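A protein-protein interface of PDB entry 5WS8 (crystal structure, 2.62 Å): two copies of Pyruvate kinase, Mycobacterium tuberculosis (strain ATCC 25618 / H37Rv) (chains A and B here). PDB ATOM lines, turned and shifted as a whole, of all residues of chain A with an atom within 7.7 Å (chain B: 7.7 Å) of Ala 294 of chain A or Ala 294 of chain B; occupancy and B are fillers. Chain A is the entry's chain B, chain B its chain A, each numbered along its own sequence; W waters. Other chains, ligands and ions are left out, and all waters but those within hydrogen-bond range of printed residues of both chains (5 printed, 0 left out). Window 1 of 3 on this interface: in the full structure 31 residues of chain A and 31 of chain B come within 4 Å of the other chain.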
ATOM      1  N   ARG A 245      -9.278 -29.267 -24.952  1.00  0.00           N
ATOM      2  CA  ARG A 245     -10.477 -29.387 -24.125  1.00  0.00           C
ATOM      3  C   ARG A 245     -11.359 -30.560 -24.477  1.00  0.00           C
ATOM      4  O   ARG A 245     -12.078 -31.056 -23.625  1.00  0.00           O
ATOM      5  CB  ARG A 245     -11.278 -28.098 -24.177  1.00  0.00           C
ATOM      6  CG  ARG A 245     -10.430 -26.927 -23.731  1.00  0.00           C
ATOM      7  CD  ARG A 245     -11.189 -25.633 -23.683  1.00  0.00           C
ATOM      8  NE  ARG A 245     -11.973 -25.417 -24.880  1.00  0.00           N
ATOM      9  CZ  ARG A 245     -12.846 -24.432 -25.002  1.00  0.00           C
ATOM     10  NH1 ARG A 245     -13.559 -24.325 -26.106  1.00  0.00           N
ATOM     11  NH2 ARG A 245     -13.028 -23.563 -24.005  1.00  0.00           N
ATOM     12  N   PRO A 258     -13.052 -25.617 -17.194  1.00  0.00           N
ATOM     13  CA  PRO A 258     -12.907 -24.167 -17.282  1.00  0.00           C
ATOM     14  C   PRO A 258     -11.867 -23.552 -16.338  1.00  0.00           C
ATOM     15  O   PRO A 258     -11.262 -22.572 -16.678  1.00  0.00           O
ATOM     16  CB  PRO A 258     -14.309 -23.661 -16.944  1.00  0.00           C
ATOM     17  CG  PRO A 258     -15.197 -24.726 -17.453  1.00  0.00           C
ATOM     18  CD  PRO A 258     -14.470 -26.013 -17.124  1.00  0.00           C
ATOM     19  N   THR A 279     -10.555 -26.573 -29.226  1.00  0.00           N
ATOM     20  CA  THR A 279     -11.617 -27.530 -29.372  1.00  0.00           C
ATOM     21  C   THR A 279     -12.964 -27.033 -28.930  1.00  0.00           C
ATOM     22  O   THR A 279     -13.136 -26.611 -27.802  1.00  0.00           O
ATOM     23  CB  THR A 279     -11.263 -28.839 -28.727  1.00  0.00           C
ATOM     24  OG1 THR A 279     -10.082 -29.336 -29.372  1.00  0.00           O
ATOM     25  CG2 THR A 279     -12.395 -29.822 -28.926  1.00  0.00           C
ATOM     26  N   GLN A 280     -13.902 -27.067 -29.870  1.00  0.00           N
ATOM     27  CA  GLN A 280     -15.307 -26.729 -29.642  1.00  0.00           C
ATOM     28  C   GLN A 280     -15.580 -25.259 -29.324  1.00  0.00           C
ATOM     29  O   GLN A 280     -16.596 -24.928 -28.730  1.00  0.00           O
ATOM     30  CB  GLN A 280     -15.926 -27.642 -28.569  1.00  0.00           C
ATOM     31  CG  GLN A 280     -16.258 -29.015 -29.099  1.00  0.00           C
ATOM     32  CD  GLN A 280     -16.692 -30.007 -28.041  1.00  0.00           C
ATOM     33  OE1 GLN A 280     -17.444 -29.691 -27.123  1.00  0.00           O
ATOM     34  NE2 GLN A 280     -16.239 -31.229 -28.192  1.00  0.00           N
ATOM     35  N   MET A 281     -14.708 -24.369 -29.746  1.00  0.00           N
ATOM     36  CA  MET A 281     -14.931 -22.967 -29.449  1.00  0.00           C
ATOM     37  C   MET A 281     -16.085 -22.422 -30.238  1.00  0.00           C
ATOM     38  O   MET A 281     -16.871 -21.655 -29.708  1.00  0.00           O
ATOM     39  CB  MET A 281     -13.692 -22.150 -29.717  1.00  0.00           C
ATOM     40  CG  MET A 281     -12.501 -22.661 -28.955  1.00  0.00           C
ATOM     41  SD  MET A 281     -11.375 -21.344 -28.549  1.00  0.00           S
ATOM     42  CE  MET A 281     -12.188 -20.659 -27.110  1.00  0.00           C
ATOM     43  N   LEU A 282     -16.174 -22.790 -31.513  1.00  0.00           N
ATOM     44  CA  LEU A 282     -17.327 -22.430 -32.328  1.00  0.00           C
ATOM     45  C   LEU A 282     -17.901 -23.688 -32.932  1.00  0.00           C
ATOM     46  O   LEU A 282     -18.167 -23.759 -34.128  1.00  0.00           O
ATOM     47  CB  LEU A 282     -16.931 -21.439 -33.414  1.00  0.00           C
ATOM     48  CG  LEU A 282     -16.427 -20.099 -32.882  1.00  0.00           C
ATOM     49  CD1 LEU A 282     -15.729 -19.341 -33.977  1.00  0.00           C
ATOM     50  CD2 LEU A 282     -17.528 -19.233 -32.295  1.00  0.00           C
ATOM     51  N   ASP A 283     -18.110 -24.676 -32.087  1.00  0.00           N
ATOM     52  CA  ASP A 283     -18.498 -26.016 -32.537  1.00  0.00           C
ATOM     53  C   ASP A 283     -19.708 -26.052 -33.447  1.00  0.00           C
ATOM     54  O   ASP A 283     -19.746 -26.817 -34.380  1.00  0.00           O
ATOM     55  CB  ASP A 283     -18.763 -26.927 -31.334  1.00  0.00           C
ATOM     56  CG  ASP A 283     -18.860 -28.371 -31.728  1.00  0.00           C
ATOM     57  OD1 ASP A 283     -17.843 -28.927 -32.216  1.00  0.00           O
ATOM     58  OD2 ASP A 283     -19.957 -28.940 -31.574  1.00  0.00           O
ATOM     59  N   SER A 284     -20.706 -25.240 -33.160  1.00  0.00           N
ATOM     60  CA  SER A 284     -21.930 -25.278 -33.917  1.00  0.00           C
ATOM     61  C   SER A 284     -21.752 -24.777 -35.342  1.00  0.00           C
ATOM     62  O   SER A 284     -22.647 -24.950 -36.171  1.00  0.00           O
ATOM     63  CB  SER A 284     -23.022 -24.464 -33.223  1.00  0.00           C
ATOM     64  OG  SER A 284     -22.771 -23.079 -33.330  1.00  0.00           O
ATOM     65  N   PRO A 291     -22.569 -18.758 -34.811  1.00  0.00           N
ATOM     66  CA  PRO A 291     -22.358 -19.565 -33.618  1.00  0.00           C
ATOM     67  C   PRO A 291     -23.420 -19.344 -32.542  1.00  0.00           C
ATOM     68  O   PRO A 291     -24.335 -18.513 -32.724  1.00  0.00           O
ATOM     69  CB  PRO A 291     -21.014 -19.079 -33.125  1.00  0.00           C
ATOM     70  CG  PRO A 291     -21.009 -17.641 -33.484  1.00  0.00           C
ATOM     71  CD  PRO A 291     -21.826 -17.497 -34.755  1.00  0.00           C
ATOM     72  N   THR A 292     -23.304 -20.076 -31.434  1.00  0.00           N
ATOM     73  CA  THR A 292     -24.199 -19.865 -30.302  1.00  0.00           C
ATOM     74  C   THR A 292     -23.692 -18.781 -29.377  1.00  0.00           C
ATOM     75  O   THR A 292     -22.515 -18.408 -29.383  1.00  0.00           O
ATOM     76  CB  THR A 292     -24.414 -21.136 -29.463  1.00  0.00           C
ATOM     77  OG1 THR A 292     -23.197 -21.513 -28.796  1.00  0.00           O
ATOM     78  CG2 THR A 292     -24.904 -22.283 -30.319  1.00  0.00           C
ATOM     79  N   ARG A 293     -24.574 -18.310 -28.523  1.00  0.00           N
ATOM     80  CA  ARG A 293     -24.185 -17.305 -27.587  1.00  0.00           C
ATOM     81  C   ARG A 293     -23.096 -17.833 -26.643  1.00  0.00           C
ATOM     82  O   ARG A 293     -22.240 -17.078 -26.188  1.00  0.00           O
ATOM     83  CB  ARG A 293     -25.399 -16.807 -26.820  1.00  0.00           C
ATOM     84  CG  ARG A 293     -26.511 -16.243 -27.706  1.00  0.00           C
ATOM     85  CD  ARG A 293     -26.104 -14.970 -28.438  1.00  0.00           C
ATOM     86  NE  ARG A 293     -27.187 -14.597 -29.310  1.00  0.00           N
ATOM     87  CZ  ARG A 293     -27.366 -15.080 -30.525  1.00  0.00           C
ATOM     88  NH1 ARG A 293     -26.482 -15.896 -31.067  1.00  0.00           N
ATOM     89  NH2 ARG A 293     -28.431 -14.742 -31.200  1.00  0.00           N
ATOM     90  N   ALA A 294     -23.111 -19.122 -26.362  1.00  0.00           N
ATOM     91  CA  ALA A 294     -22.092 -19.689 -25.505  1.00  0.00           C
ATOM     92  C   ALA A 294     -20.771 -19.758 -26.231  1.00  0.00           C
ATOM     93  O   ALA A 294     -19.705 -19.625 -25.642  1.00  0.00           O
ATOM     94  CB  ALA A 294     -22.498 -21.070 -25.045  1.00  0.00           C
ATOM     95  N   GLU A 295     -20.828 -20.011 -27.517  1.00  0.00           N
ATOM     96  CA  GLU A 295     -19.615 -20.095 -28.276  1.00  0.00           C
ATOM     97  C   GLU A 295     -18.944 -18.725 -28.383  1.00  0.00           C
ATOM     98  O   GLU A 295     -17.772 -18.586 -28.056  1.00  0.00           O
ATOM     99  CB  GLU A 295     -19.896 -20.735 -29.618  1.00  0.00           C
ATOM    100  CG  GLU A 295     -20.057 -22.228 -29.451  1.00  0.00           C
ATOM    101  CD  GLU A 295     -20.776 -22.916 -30.583  1.00  0.00           C
ATOM    102  OE1 GLU A 295     -21.280 -22.220 -31.506  1.00  0.00           O
ATOM    103  OE2 GLU A 295     -20.850 -24.180 -30.513  1.00  0.00           O
ATOM    104  N   ALA A 296     -19.702 -17.697 -28.742  1.00  0.00           N
ATOM    105  CA  ALA A 296     -19.141 -16.332 -28.748  1.00  0.00           C
ATOM    106  C   ALA A 296     -18.514 -15.995 -27.380  1.00  0.00           C
ATOM    107  O   ALA A 296     -17.443 -15.410 -27.314  1.00  0.00           O
ATOM    108  CB  ALA A 296     -20.207 -15.299 -29.115  1.00  0.00           C
ATOM    109  N   SER A 297     -19.198 -16.375 -26.306  1.00  0.00           N
ATOM    110  CA  SER A 297     -18.739 -16.107 -24.954  1.00  0.00           C
ATOM    111  C   SER A 297     -17.453 -16.842 -24.642  1.00  0.00           C
ATOM    112  O   SER A 297     -16.554 -16.305 -23.970  1.00  0.00           O
ATOM    113  CB  SER A 297     -19.800 -16.518 -23.926  1.00  0.00           C
ATOM    114  OG  SER A 297     -19.345 -16.217 -22.621  1.00  0.00           O
ATOM    115  N   ASP A 298     -17.367 -18.069 -25.124  1.00  0.00           N
ATOM    116  CA  ASP A 298     -16.221 -18.904 -24.861  1.00  0.00           C
ATOM    117  C   ASP A 298     -14.958 -18.320 -25.506  1.00  0.00           C
ATOM    118  O   ASP A 298     -13.883 -18.304 -24.899  1.00  0.00           O
ATOM    119  CB  ASP A 298     -16.509 -20.303 -25.387  1.00  0.00           C
ATOM    120  CG  ASP A 298     -15.370 -21.262 -25.172  1.00  0.00           C
ATOM    121  OD1 ASP A 298     -14.784 -21.289 -24.069  1.00  0.00           O
ATOM    122  OD2 ASP A 298     -15.079 -22.016 -26.119  1.00  0.00           O
ATOM    123  N   VAL A 299     -15.093 -17.811 -26.723  1.00  0.00           N
ATOM    124  CA  VAL A 299     -13.973 -17.219 -27.428  1.00  0.00           C
ATOM    125  C   VAL A 299     -13.567 -15.917 -26.774  1.00  0.00           C
ATOM    126  O   VAL A 299     -12.387 -15.667 -26.565  1.00  0.00           O
ATOM    127  CB  VAL A 299     -14.337 -16.977 -28.904  1.00  0.00           C
ATOM    128  CG1 VAL A 299     -13.342 -16.051 -29.605  1.00  0.00           C
ATOM    129  CG2 VAL A 299     -14.435 -18.313 -29.630  1.00  0.00           C
ATOM    130  N   ALA A 300     -14.541 -15.079 -26.454  1.00  0.00           N
ATOM    131  CA  ALA A 300     -14.258 -13.820 -25.767  1.00  0.00           C
ATOM    132  C   ALA A 300     -13.554 -14.082 -24.454  1.00  0.00           C
ATOM    133  O   ALA A 300     -12.610 -13.383 -24.116  1.00  0.00           O
ATOM    134  CB  ALA A 300     -15.531 -13.021 -25.517  1.00  0.00           C
ATOM    135  N   ASN A 301     -14.000 -15.103 -23.725  1.00  0.00           N
ATOM    136  CA  ASN A 301     -13.417 -15.400 -22.436  1.00  0.00           C
ATOM    137  C   ASN A 301     -12.018 -15.966 -22.525  1.00  0.00           C
ATOM    138  O   ASN A 301     -11.187 -15.646 -21.691  1.00  0.00           O
ATOM    139  CB  ASN A 301     -14.338 -16.286 -21.588  1.00  0.00           C
ATOM    140  CG  ASN A 301     -15.357 -15.459 -20.814  1.00  0.00           C
ATOM    141  OD1 ASN A 301     -14.982 -14.691 -19.923  1.00  0.00           O
ATOM    142  ND2 ASN A 301     -16.641 -15.572 -21.178  1.00  0.00           N
ATOM    143  N   ARG B 245     -29.673 -13.020 -24.153  1.00  0.00           N
ATOM    144  CA  ARG B 245     -28.631 -13.077 -25.170  1.00  0.00           C
ATOM    145  C   ARG B 245     -29.120 -13.551 -26.519  1.00  0.00           C
ATOM    146  O   ARG B 245     -28.531 -13.207 -27.528  1.00  0.00           O
ATOM    147  CB  ARG B 245     -27.491 -13.957 -24.694  1.00  0.00           C
ATOM    148  CG  ARG B 245     -26.935 -13.463 -23.383  1.00  0.00           C
ATOM    149  CD  ARG B 245     -25.746 -14.246 -22.914  1.00  0.00           C
ATOM    150  NE  ARG B 245     -25.965 -15.674 -22.999  1.00  0.00           N
ATOM    151  CZ  ARG B 245     -25.015 -16.567 -22.788  1.00  0.00           C
ATOM    152  NH1 ARG B 245     -25.281 -17.854 -22.919  1.00  0.00           N
ATOM    153  NH2 ARG B 245     -23.794 -16.176 -22.442  1.00  0.00           N
ATOM    154  N   PRO B 258     -20.728 -10.519 -25.463  1.00  0.00           N
ATOM    155  CA  PRO B 258     -19.983 -10.917 -24.271  1.00  0.00           C
ATOM    156  C   PRO B 258     -19.555  -9.771 -23.354  1.00  0.00           C
ATOM    157  O   PRO B 258     -19.489  -9.949 -22.169  1.00  0.00           O
ATOM    158  CB  PRO B 258     -18.748 -11.618 -24.852  1.00  0.00           C
ATOM    159  CG  PRO B 258     -19.221 -12.188 -26.126  1.00  0.00           C
ATOM    160  CD  PRO B 258     -20.230 -11.206 -26.665  1.00  0.00           C
ATOM    161  N   THR B 279     -30.066 -17.778 -22.012  1.00  0.00           N
ATOM    162  CA  THR B 279     -30.209 -18.255 -23.359  1.00  0.00           C
ATOM    163  C   THR B 279     -28.969 -18.868 -23.927  1.00  0.00           C
ATOM    164  O   THR B 279     -27.924 -18.238 -23.971  1.00  0.00           O
ATOM    165  CB  THR B 279     -30.772 -17.192 -24.262  1.00  0.00           C
ATOM    166  OG1 THR B 279     -32.065 -16.839 -23.759  1.00  0.00           O
ATOM    167  CG2 THR B 279     -30.915 -17.739 -25.671  1.00  0.00           C
ATOM    168  N   GLN B 280     -29.109 -20.127 -24.333  1.00  0.00           N
ATOM    169  CA  GLN B 280     -28.053 -20.893 -25.005  1.00  0.00           C
ATOM    170  C   GLN B 280     -26.833 -21.221 -24.142  1.00  0.00           C
ATOM    171  O   GLN B 280     -25.761 -21.488 -24.656  1.00  0.00           O
ATOM    172  CB  GLN B 280     -27.613 -20.205 -26.310  1.00  0.00           C
ATOM    173  CG  GLN B 280     -28.591 -20.401 -27.439  1.00  0.00           C
ATOM    174  CD  GLN B 280     -28.285 -19.576 -28.671  1.00  0.00           C
ATOM    175  OE1 GLN B 280     -27.139 -19.416 -29.084  1.00  0.00           O
ATOM    176  NE2 GLN B 280     -29.325 -19.057 -29.272  1.00  0.00           N
ATOM    177  N   MET B 281     -26.997 -21.257 -22.840  1.00  0.00           N
ATOM    178  CA  MET B 281     -25.867 -21.570 -21.991  1.00  0.00           C
ATOM    179  C   MET B 281     -25.464 -23.020 -22.129  1.00  0.00           C
ATOM    180  O   MET B 281     -24.288 -23.315 -22.170  1.00  0.00           O
ATOM    181  CB  MET B 281     -26.171 -21.252 -20.554  1.00  0.00           C
ATOM    182  CG  MET B 281     -26.588 -19.815 -20.363  1.00  0.00           C
ATOM    183  SD  MET B 281     -26.118 -19.209 -18.748  1.00  0.00           S
ATOM    184  CE  MET B 281     -24.410 -18.821 -19.058  1.00  0.00           C
ATOM    185  N   LEU B 282     -26.441 -23.921 -22.184  1.00  0.00           N
ATOM    186  CA  LEU B 282     -26.162 -25.324 -22.468  1.00  0.00           C
ATOM    187  C   LEU B 282     -27.016 -25.760 -23.629  1.00  0.00           C
ATOM    188  O   LEU B 282     -27.677 -26.790 -23.585  1.00  0.00           O
ATOM    189  CB  LEU B 282     -26.430 -26.194 -21.252  1.00  0.00           C
ATOM    190  CG  LEU B 282     -25.564 -25.860 -20.032  1.00  0.00           C
ATOM    191  CD1 LEU B 282     -26.169 -26.472 -18.800  1.00  0.00           C
ATOM    192  CD2 LEU B 282     -24.122 -26.317 -20.188  1.00  0.00           C
ATOM    193  N   ASP B 283     -26.980 -24.966 -24.688  1.00  0.00           N
ATOM    194  CA  ASP B 283     -27.877 -25.149 -25.827  1.00  0.00           C
ATOM    195  C   ASP B 283     -27.869 -26.542 -26.414  1.00  0.00           C
ATOM    196  O   ASP B 283     -28.900 -27.048 -26.800  1.00  0.00           O
ATOM    197  CB  ASP B 283     -27.544 -24.154 -26.936  1.00  0.00           C
ATOM    198  CG  ASP B 283     -28.623 -24.093 -27.992  1.00  0.00           C
ATOM    199  OD1 ASP B 283     -29.764 -23.695 -27.665  1.00  0.00           O
ATOM    200  OD2 ASP B 283     -28.336 -24.473 -29.135  1.00  0.00           O
ATOM    201  N   SER B 284     -26.705 -27.152 -26.511  1.00  0.00           N
ATOM    202  CA  SER B 284     -26.592 -28.442 -27.146  1.00  0.00           C
ATOM    203  C   SER B 284     -27.261 -29.550 -26.358  1.00  0.00           C
ATOM    204  O   SER B 284     -27.431 -30.647 -26.877  1.00  0.00           O
ATOM    205  CB  SER B 284     -25.129 -28.806 -27.380  1.00  0.00           C
ATOM    206  OG  SER B 284     -24.493 -29.140 -26.161  1.00  0.00           O
ATOM    207  N   PRO B 291     -22.927 -31.349 -22.493  1.00  0.00           N
ATOM    208  CA  PRO B 291     -22.771 -30.103 -23.218  1.00  0.00           C
ATOM    209  C   PRO B 291     -21.437 -30.002 -23.957  1.00  0.00           C
ATOM    210  O   PRO B 291     -20.611 -30.917 -23.875  1.00  0.00           O
ATOM    211  CB  PRO B 291     -22.847 -29.068 -22.111  1.00  0.00           C
ATOM    212  CG  PRO B 291     -22.214 -29.748 -20.955  1.00  0.00           C
ATOM    213  CD  PRO B 291     -22.524 -31.220 -21.091  1.00  0.00           C
ATOM    214  N   THR B 292     -21.236 -28.900 -24.670  1.00  0.00           N
ATOM    215  CA  THR B 292     -19.950 -28.652 -25.317  1.00  0.00           C
ATOM    216  C   THR B 292     -18.977 -27.955 -24.383  1.00  0.00           C
ATOM    217  O   THR B 292     -19.344 -27.364 -23.370  1.00  0.00           O
ATOM    218  CB  THR B 292     -20.080 -27.782 -26.591  1.00  0.00           C
ATOM    219  OG1 THR B 292     -20.493 -26.445 -26.252  1.00  0.00           O
ATOM    220  CG2 THR B 292     -21.067 -28.391 -27.568  1.00  0.00           C
ATOM    221  N   ARG B 293     -17.721 -27.968 -24.764  1.00  0.00           N
ATOM    222  CA  ARG B 293     -16.726 -27.327 -23.963  1.00  0.00           C
ATOM    223  C   ARG B 293     -16.992 -25.827 -23.881  1.00  0.00           C
ATOM    224  O   ARG B 293     -16.679 -25.193 -22.874  1.00  0.00           O
ATOM    225  CB  ARG B 293     -15.345 -27.609 -24.522  1.00  0.00           C
ATOM    226  CG  ARG B 293     -14.995 -29.087 -24.611  1.00  0.00           C
ATOM    227  CD  ARG B 293     -14.878 -29.740 -23.242  1.00  0.00           C
ATOM    228  NE  ARG B 293     -14.649 -31.149 -23.425  1.00  0.00           N
ATOM    229  CZ  ARG B 293     -15.605 -32.033 -23.638  1.00  0.00           C
ATOM    230  NH1 ARG B 293     -16.888 -31.672 -23.629  1.00  0.00           N
ATOM    231  NH2 ARG B 293     -15.276 -33.282 -23.850  1.00  0.00           N
ATOM    232  N   ALA B 294     -17.585 -25.257 -24.919  1.00  0.00           N
ATOM    233  CA  ALA B 294     -17.882 -23.840 -24.895  1.00  0.00           C
ATOM    234  C   ALA B 294     -19.030 -23.572 -23.951  1.00  0.00           C
ATOM    235  O   ALA B 294     -19.093 -22.531 -23.302  1.00  0.00           O
ATOM    236  CB  ALA B 294     -18.235 -23.350 -26.283  1.00  0.00           C
ATOM    237  N   GLU B 295     -19.971 -24.494 -23.904  1.00  0.00           N
ATOM    238  CA  GLU B 295     -21.100 -24.313 -23.049  1.00  0.00           C
ATOM    239  C   GLU B 295     -20.681 -24.376 -21.587  1.00  0.00           C
ATOM    240  O   GLU B 295     -20.983 -23.464 -20.817  1.00  0.00           O
ATOM    241  CB  GLU B 295     -22.179 -25.310 -23.408  1.00  0.00           C
ATOM    242  CG  GLU B 295     -22.890 -24.856 -24.665  1.00  0.00           C
ATOM    243  CD  GLU B 295     -23.654 -25.931 -25.390  1.00  0.00           C
ATOM    244  OE1 GLU B 295     -23.564 -27.122 -24.992  1.00  0.00           O
ATOM    245  OE2 GLU B 295     -24.334 -25.558 -26.385  1.00  0.00           O
ATOM    246  N   ALA B 296     -19.920 -25.397 -21.210  1.00  0.00           N
ATOM    247  CA  ALA B 296     -19.405 -25.465 -19.833  1.00  0.00           C
ATOM    248  C   ALA B 296     -18.648 -24.172 -19.476  1.00  0.00           C
ATOM    249  O   ALA B 296     -18.791 -23.645 -18.384  1.00  0.00           O
ATOM    250  CB  ALA B 296     -18.500 -26.679 -19.650  1.00  0.00           C
ATOM    251  N   SER B 297     -17.855 -23.674 -20.409  1.00  0.00           N
ATOM    252  CA  SER B 297     -17.066 -22.468 -20.195  1.00  0.00           C
ATOM    253  C   SER B 297     -17.952 -21.246 -20.017  1.00  0.00           C
ATOM    254  O   SER B 297     -17.655 -20.356 -19.216  1.00  0.00           O
ATOM    255  CB  SER B 297     -16.119 -22.235 -21.377  1.00  0.00           C
ATOM    256  OG  SER B 297     -15.373 -21.064 -21.189  1.00  0.00           O
ATOM    257  N   ASP B 298     -19.029 -21.201 -20.780  1.00  0.00           N
ATOM    258  CA  ASP B 298     -19.926 -20.063 -20.758  1.00  0.00           C
ATOM    259  C   ASP B 298     -20.627 -19.961 -19.396  1.00  0.00           C
ATOM    260  O   ASP B 298     -20.771 -18.875 -18.841  1.00  0.00           O
ATOM    261  CB  ASP B 298     -20.930 -20.211 -21.900  1.00  0.00           C
ATOM    262  CG  ASP B 298     -21.961 -19.108 -21.931  1.00  0.00           C
ATOM    263  OD1 ASP B 298     -21.599 -17.921 -21.801  1.00  0.00           O
ATOM    264  OD2 ASP B 298     -23.148 -19.437 -22.108  1.00  0.00           O
ATOM    265  N   VAL B 299     -21.029 -21.097 -18.847  1.00  0.00           N
ATOM    266  CA  VAL B 299     -21.673 -21.130 -17.544  1.00  0.00           C
ATOM    267  C   VAL B 299     -20.682 -20.767 -16.455  1.00  0.00           C
ATOM    268  O   VAL B 299     -20.992 -19.978 -15.571  1.00  0.00           O
ATOM    269  CB  VAL B 299     -22.271 -22.527 -17.271  1.00  0.00           C
ATOM    270  CG1 VAL B 299     -22.651 -22.714 -15.804  1.00  0.00           C
ATOM    271  CG2 VAL B 299     -23.476 -22.736 -18.161  1.00  0.00           C
ATOM    272  N   ALA B 300     -19.499 -21.355 -16.507  1.00  0.00           N
ATOM    273  CA  ALA B 300     -18.453 -21.030 -15.535  1.00  0.00           C
ATOM    274  C   ALA B 300     -18.134 -19.552 -15.566  1.00  0.00           C
ATOM    275  O   ALA B 300     -17.973 -18.939 -14.528  1.00  0.00           O
ATOM    276  CB  ALA B 300     -17.181 -21.830 -15.795  1.00  0.00           C
ATOM    277  N   ASN B 301     -18.069 -18.980 -16.762  1.00  0.00           N
ATOM    278  CA  ASN B 301     -17.727 -17.588 -16.902  1.00  0.00           C
ATOM    279  C   ASN B 301     -18.812 -16.648 -16.434  1.00  0.00           C
ATOM    280  O   ASN B 301     -18.510 -15.616 -15.856  1.00  0.00           O
ATOM    281  CB  ASN B 301     -17.253 -17.262 -18.328  1.00  0.00           C
ATOM    282  CG  ASN B 301     -15.761 -17.528 -18.495  1.00  0.00           C
ATOM    283  OD1 ASN B 301     -14.940 -16.830 -17.881  1.00  0.00           O
ATOM    284  ND2 ASN B 301     -15.397 -18.572 -19.260  1.00  0.00           N
HETATM  285  O   HOH W   1     -13.100 -19.931 -22.914  1.00  0.00           O
HETATM  286  O   HOH W   2     -19.569 -13.345 -21.510  1.00  0.00           O
HETATM  287  O   HOH W   3     -20.908 -16.326 -19.913  1.00  0.00           O
HETATM  288  O   HOH W   4     -22.892 -25.123 -28.682  1.00  0.00           O
HETATM  289  O   HOH W   5     -15.508 -14.354 -16.601  1.00  0.00           O
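O of Arg 245 of chain B is in hydrogen-bond range of NE of Arg 293 of chain A.
The side-chain amide oxygen of Gln 280 of chain B is in hydrogen-bond range of the backbone NH of Arg 293 of chain A (2.8 Å).
The backbone carbonyl oxygen (O) of Arg 245 of chain A is in hydrogen-bond range of the guanidinium group (NE) of Arg 293 of chain B (2.6 Å).
N of Arg 293 of chain B is in hydrogen-bond range of OE1 of Gln 280 of chain A, 2.9 Å away.
The side-chain hydroxyl (OG) of Ser 297 of chain B sits at hydrogen-bond distance from the side-chain carboxylate (OD1) of Asp 298 of chain A, 2.9 Å away.
The side-chain carboxylate (OD1) of Asp 298 of chain B is in hydrogen-bond range of the side-chain hydroxyl (OG) of Ser 297 of chain A, 2.9 Å away.
The side-chain amide oxygen (OD1) of Asn 301 of chain B lies close to the side-chain amide oxygen (OD1) of Asn 301 of chain A (3.0 Å).
NH1 of Arg 245 of chain B lies within salt-bridge range of OD2 of Asp 298 of chain B, 2.8 Å away.
The backbone NH (N) of Thr 292 of chain B sits at hydrogen-bond distance from the side-chain carboxylate (OE1) of Glu 295 of chain B (2.9 Å).
The backbone carbonyl oxygen (O) of Ser 297 of chain B is in hydrogen-bond range of the side-chain amide nitrogen (ND2) of Asn 301 of chain B.
The backbone NH (N) of Asp 283 of chain A lies within hydrogen-bond range of the side-chain carboxylate (OE2) of Glu 295 of chain A, at 3.2 Å.
OE1 of Glu 295 of chain A sits at hydrogen-bond distance from OG of Ser 284 of chain A.
The side-chain hydroxyl (OG1) of Thr 292 of chain A lies close to the backbone NH (N) of Ala 294 of chain A, 3.4 Å away.
Arg 245 of chain A touches Arg 293 of chain B, and with the chains exchanged Arg 293 of chain A touches Arg 245 of chain B.
Gln 280 of chain A touches Arg 293 of chain B, and with the chains exchanged Arg 293 of chain A touches Gln 280 of chain B.
Gln 280 of chain A touches Ala 294 of chain B, and with the chains exchanged Ala 294 of chain A touches Gln 280 of chain B.
Ala 294 of chain A touches Asp 298 of chain B, and with the chains exchanged Asp 298 of chain A touches Ala 294 of chain B.
Ala 296 of chain B touches Pro 258 of chain A (O to CG, 3.9 Å).
Pro 258 of chain A touches Ala 300 of chain B (CB to CB, 3.6 Å).
OE1 of Gln 280 of chain A touches CA of Thr 292 of chain B, at 3.3 Å.
Gln 280 of chain A touches Ala 294 of chain B.
Gln 280 of chain B touches Thr 292 of chain A.
Ala 294 of chain A touches Glu 295 of chain B (CB to CG, 3.8 Å).
CB of Ala 294 of chain A touches OD2 of Asp 298 of chain B, at 3.4 Å.
O of Ala 296 of chain A touches CG of Pro 258 of chain B, at 3.9 Å.
CB of Ala 294 of chain B touches OD2 of Asp 298 of chain A, 3.4 Å away.
CB of Pro 258 of chain B touches CB of Ala 300 of chain A (3.6 Å).
Water W1 bridges OD1 of Asp 298 of chain A (2.5 Å) and OG of Ser 297 of chain B (3.1 Å).
Water W3 bridges the side-chain carboxylate (OD1) of Asp 298 of chain B (2.6 Å) and the side-chain hydroxyl (OG) of Ser 297 of chain A (3.1 Å).
Water W4 bridges OE2 of Glu 295 of chain B (2.7 Å) and OE2 of Glu 295 of chain A (2.9 Å).
Water W5 lies within hydrogen-bond range of OD1 of Asn 301 of chain B (2.8 Å) and OD1 of Asn 301 of chain A (3.4 Å).
Water W2 lies within hydrogen-bond range of the side-chain hydroxyl of Ser 297 of chain A (3.1 Å) and the backbone carbonyl oxygen of Pro 258 of chain B (3.5 Å).
Of the 19 printed residues of chain A, 12 touch a printed residue of chain B.
Of the 19 printed residues of chain B, 12 touch a printed residue of chain A.
Hydrophobic or aromatic side chains of chain B within 4 Å of the printed part of chain A: Pro 258, Ala 294 and Ala 300.
Among the printed residues, 20 pairs touch across the chains.
Ala 294 of chain A touches just these residues of chain B: Gln 280, Ala 294, Glu 295 and Asp 298.
Of chain A, only Gln 280, Ala 294, Glu 295 and Asp 298 come within 4 Å of Ala 294 of chain B.
Of the printed residues of chain A, Ala 296 of chain B touches Pro 258 (3.9 Å).
Printed residues of chain A within 4 Å of Thr 292 of chain B: Gln 280.
The nearest residue of chain B that does not touch Ala 294 of chain A is Met 281 of chain B (4.1 Å).
The nearest residue of chain A that does not touch Ala 294 of chain B is Met 281 of chain A (4.1 Å).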
